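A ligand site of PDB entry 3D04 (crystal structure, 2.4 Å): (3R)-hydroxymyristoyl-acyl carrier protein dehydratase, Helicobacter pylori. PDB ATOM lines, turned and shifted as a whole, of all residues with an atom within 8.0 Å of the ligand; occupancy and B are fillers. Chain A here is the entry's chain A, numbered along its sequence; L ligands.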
ATOM      1  N   GLN A  37       5.453 -23.170 -13.908  1.00  0.00           N
ATOM      2  CA  GLN A  37       6.710 -23.835 -13.554  1.00  0.00           C
ATOM      3  C   GLN A  37       6.512 -25.344 -13.623  1.00  0.00           C
ATOM      4  O   GLN A  37       5.750 -25.901 -12.842  1.00  0.00           O
ATOM      5  CB  GLN A  37       7.174 -23.396 -12.158  1.00  0.00           C
ATOM      6  CG  GLN A  37       8.650 -23.684 -11.849  1.00  0.00           C
ATOM      7  CD  GLN A  37       9.617 -22.914 -12.752  1.00  0.00           C
ATOM      8  OE1 GLN A  37      10.652 -23.450 -13.173  1.00  0.00           O
ATOM      9  NE2 GLN A  37       9.294 -21.646 -13.051  1.00  0.00           N
ATOM     10  N   ALA A  38       7.187 -25.990 -14.573  1.00  0.00           N
ATOM     11  CA  ALA A  38       7.030 -27.426 -14.843  1.00  0.00           C
ATOM     12  C   ALA A  38       7.197 -28.284 -13.589  1.00  0.00           C
ATOM     13  O   ALA A  38       8.129 -28.074 -12.804  1.00  0.00           O
ATOM     14  CB  ALA A  38       8.006 -27.881 -15.924  1.00  0.00           C
ATOM     15  N   ASN A  39       6.270 -29.228 -13.400  1.00  0.00           N
ATOM     16  CA  ASN A  39       6.252 -30.151 -12.249  1.00  0.00           C
ATOM     17  C   ASN A  39       6.106 -29.473 -10.888  1.00  0.00           C
ATOM     18  O   ASN A  39       6.237 -30.129  -9.853  1.00  0.00           O
ATOM     19  CB  ASN A  39       7.499 -31.058 -12.217  1.00  0.00           C
ATOM     20  CG  ASN A  39       7.737 -31.779 -13.534  1.00  0.00           C
ATOM     21  OD1 ASN A  39       8.718 -31.528 -14.214  1.00  0.00           O
ATOM     22  ND2 ASN A  39       6.837 -32.674 -13.886  1.00  0.00           N
ATOM     23  N   GLN A  40       5.820 -28.173 -10.893  1.00  0.00           N
ATOM     24  CA  GLN A  40       5.783 -27.416  -9.641  1.00  0.00           C
ATOM     25  C   GLN A  40       4.493 -26.643  -9.434  1.00  0.00           C
ATOM     26  O   GLN A  40       3.752 -26.897  -8.476  1.00  0.00           O
ATOM     27  CB  GLN A  40       6.988 -26.479  -9.534  1.00  0.00           C
ATOM     28  CG  GLN A  40       8.318 -27.186  -9.338  1.00  0.00           C
ATOM     29  CD  GLN A  40       9.364 -26.281  -8.748  1.00  0.00           C
ATOM     30  OE1 GLN A  40      10.402 -26.029  -9.356  1.00  0.00           O
ATOM     31  NE2 GLN A  40       9.107 -25.773  -7.551  1.00  0.00           N
ATOM     32  N   LYS A  41       4.219 -25.699 -10.341  1.00  0.00           N
ATOM     33  CA  LYS A  41       3.049 -24.842 -10.194  1.00  0.00           C
ATOM     34  C   LYS A  41       2.540 -24.138 -11.445  1.00  0.00           C
ATOM     35  O   LYS A  41       3.240 -24.020 -12.461  1.00  0.00           O
ATOM     36  CB  LYS A  41       3.257 -23.819  -9.067  1.00  0.00           C
ATOM     37  CG  LYS A  41       4.098 -22.614  -9.395  1.00  0.00           C
ATOM     38  CD  LYS A  41       3.652 -21.476  -8.473  1.00  0.00           C
ATOM     39  CE  LYS A  41       4.576 -20.271  -8.549  1.00  0.00           C
ATOM     40  NZ  LYS A  41       3.964 -19.132  -7.773  1.00  0.00           N
ATOM     41  N   ILE A  42       1.288 -23.680 -11.344  1.00  0.00           N
ATOM     42  CA  ILE A  42       0.632 -22.860 -12.344  1.00  0.00           C
ATOM     43  C   ILE A  42      -0.195 -21.768 -11.649  1.00  0.00           C
ATOM     44  O   ILE A  42      -0.819 -22.002 -10.613  1.00  0.00           O
ATOM     45  CB  ILE A  42      -0.254 -23.727 -13.320  1.00  0.00           C
ATOM     46  CG1 ILE A  42      -0.841 -22.855 -14.442  1.00  0.00           C
ATOM     47  CG2 ILE A  42      -1.330 -24.509 -12.553  1.00  0.00           C
ATOM     48  CD1 ILE A  42      -1.504 -23.634 -15.558  1.00  0.00           C
ATOM     49  N   LEU A 123      -2.399 -23.385  -8.387  1.00  0.00           N
ATOM     50  CA  LEU A 123      -2.232 -24.816  -8.161  1.00  0.00           C
ATOM     51  C   LEU A 123      -0.761 -25.183  -7.991  1.00  0.00           C
ATOM     52  O   LEU A 123       0.089 -24.702  -8.754  1.00  0.00           O
ATOM     53  CB  LEU A 123      -2.861 -25.644  -9.289  1.00  0.00           C
ATOM     54  CG  LEU A 123      -4.388 -25.852  -9.341  1.00  0.00           C
ATOM     55  CD1 LEU A 123      -4.918 -26.601  -8.121  1.00  0.00           C
ATOM     56  CD2 LEU A 123      -5.146 -24.526  -9.521  1.00  0.00           C
ATOM     57  N   GLU A 124      -0.493 -26.023  -6.998  1.00  0.00           N
ATOM     58  CA  GLU A 124       0.846 -26.536  -6.736  1.00  0.00           C
ATOM     59  C   GLU A 124       0.824 -28.056  -6.917  1.00  0.00           C
ATOM     60  O   GLU A 124      -0.184 -28.699  -6.632  1.00  0.00           O
ATOM     61  CB  GLU A 124       1.280 -26.195  -5.299  1.00  0.00           C
ATOM     62  CG  GLU A 124       0.917 -24.770  -4.816  1.00  0.00           C
ATOM     63  CD  GLU A 124       2.038 -23.744  -4.962  1.00  0.00           C
ATOM     64  OE1 GLU A 124       2.242 -22.969  -4.004  1.00  0.00           O
ATOM     65  OE2 GLU A 124       2.730 -23.711  -5.999  1.00  0.00           O
ATOM     66  N   VAL A 125       1.938 -28.615  -7.391  1.00  0.00           N
ATOM     67  CA  VAL A 125       2.067 -30.066  -7.539  1.00  0.00           C
ATOM     68  C   VAL A 125       2.489 -30.730  -6.226  1.00  0.00           C
ATOM     69  O   VAL A 125       3.604 -30.520  -5.742  1.00  0.00           O
ATOM     70  CB  VAL A 125       3.047 -30.455  -8.675  1.00  0.00           C
ATOM     71  CG1 VAL A 125       3.199 -31.981  -8.771  1.00  0.00           C
ATOM     72  CG2 VAL A 125       2.596 -29.877  -9.999  1.00  0.00           C
ATOM     73  N   LEU A 126       1.596 -31.528  -5.662  1.00  0.00           N
ATOM     74  CA  LEU A 126       1.835 -32.215  -4.406  1.00  0.00           C
ATOM     75  C   LEU A 126       2.542 -33.553  -4.616  1.00  0.00           C
ATOM     76  O   LEU A 126       3.415 -33.925  -3.841  1.00  0.00           O
ATOM     77  CB  LEU A 126       0.528 -32.407  -3.634  1.00  0.00           C
ATOM     78  CG  LEU A 126      -0.288 -31.143  -3.331  1.00  0.00           C
ATOM     79  CD1 LEU A 126      -1.620 -31.521  -2.702  1.00  0.00           C
ATOM     80  CD2 LEU A 126       0.481 -30.189  -2.419  1.00  0.00           C
ATOM     81  N   LYS A 127       2.158 -34.241  -5.687  1.00  0.00           N
ATOM     82  CA  LYS A 127       2.773 -35.512  -6.073  1.00  0.00           C
ATOM     83  C   LYS A 127       2.527 -35.795  -7.558  1.00  0.00           C
ATOM     84  O   LYS A 127       1.465 -35.496  -8.105  1.00  0.00           O
ATOM     85  CB  LYS A 127       2.196 -36.648  -5.223  1.00  0.00           C
ATOM     86  CG  LYS A 127       3.010 -37.925  -5.262  1.00  0.00           C
ATOM     87  CD  LYS A 127       2.289 -39.060  -4.570  1.00  0.00           C
ATOM     88  CE  LYS A 127       3.015 -40.385  -4.789  1.00  0.00           C
ATOM     89  NZ  LYS A 127       2.306 -41.507  -4.111  1.00  0.00           N
ATOM     90  N   GLN A 134      -1.263 -35.338  -8.429  1.00  0.00           N
ATOM     91  CA  GLN A 134      -1.976 -34.729  -7.299  1.00  0.00           C
ATOM     92  C   GLN A 134      -1.592 -33.272  -7.192  1.00  0.00           C
ATOM     93  O   GLN A 134      -0.420 -32.938  -7.045  1.00  0.00           O
ATOM     94  CB  GLN A 134      -1.653 -35.420  -5.988  1.00  0.00           C
ATOM     95  CG  GLN A 134      -2.306 -36.770  -5.818  1.00  0.00           C
ATOM     96  CD  GLN A 134      -1.881 -37.442  -4.525  1.00  0.00           C
ATOM     97  OE1 GLN A 134      -2.007 -36.855  -3.448  1.00  0.00           O
ATOM     98  NE2 GLN A 134      -1.376 -38.672  -4.623  1.00  0.00           N
ATOM     99  N   VAL A 135      -2.610 -32.414  -7.255  1.00  0.00           N
ATOM    100  CA  VAL A 135      -2.431 -30.975  -7.127  1.00  0.00           C
ATOM    101  C   VAL A 135      -3.354 -30.426  -6.052  1.00  0.00           C
ATOM    102  O   VAL A 135      -4.413 -30.994  -5.785  1.00  0.00           O
ATOM    103  CB  VAL A 135      -2.677 -30.222  -8.475  1.00  0.00           C
ATOM    104  CG1 VAL A 135      -1.693 -30.677  -9.549  1.00  0.00           C
ATOM    105  CG2 VAL A 135      -4.107 -30.420  -8.944  1.00  0.00           C
ATOM    106  N   GLY A 136      -2.943 -29.322  -5.449  1.00  0.00           N
ATOM    107  CA  GLY A 136      -3.729 -28.640  -4.439  1.00  0.00           C
ATOM    108  C   GLY A 136      -3.457 -27.161  -4.578  1.00  0.00           C
ATOM    109  O   GLY A 136      -2.444 -26.766  -5.156  1.00  0.00           O
HETATM  110  C1  LIG L   1       5.063 -26.349  -4.489  1.00  0.00           C
HETATM  111  C2  LIG L   1       4.806 -27.732  -4.486  1.00  0.00           C
HETATM  112  C3  LIG L   1       4.042 -28.298  -3.457  1.00  0.00           C
HETATM  113  C4  LIG L   1       3.544 -27.493  -2.429  1.00  0.00           C
HETATM  114  C5  LIG L   1       3.795 -26.128  -2.425  1.00  0.00           C
HETATM  115  C6  LIG L   1       4.559 -25.563  -3.453  1.00  0.00           C
HETATM  116  C7  LIG L   1       5.846 -25.774  -5.509  1.00  0.00           C
HETATM  117  N1  LIG L   1       5.566 -24.604  -6.040  1.00  0.00           N
HETATM  118  N2  LIG L   1       6.924 -26.400  -5.952  1.00  0.00           N
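The side-chain amide nitrogen (NE2) of Gln 40 lies close to a nitrogen (N2) of the ligand (2.8 Å).
N1 of the ligand lies within salt-bridge range of OE2 of Glu 124.
N of Val 125 sits at hydrogen-bond distance from O of Gln 40 (2.7 Å).
The backbone NH (N) of Glu 124 is in hydrogen-bond range of the backbone carbonyl oxygen (O) of Gly 136 (2.8 Å).
Lys 41 touches the ligand (CB to N1, 3.9 Å).
Val 125 touches the ligand (O to C3, 3.2 Å).
Four residues have an atom within 4 Å of the ligand: Gln 40, Lys 41, Glu 124 and Val 125.
Along chain A the residues within 4 Å of the ligand span positions 40 to 125.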
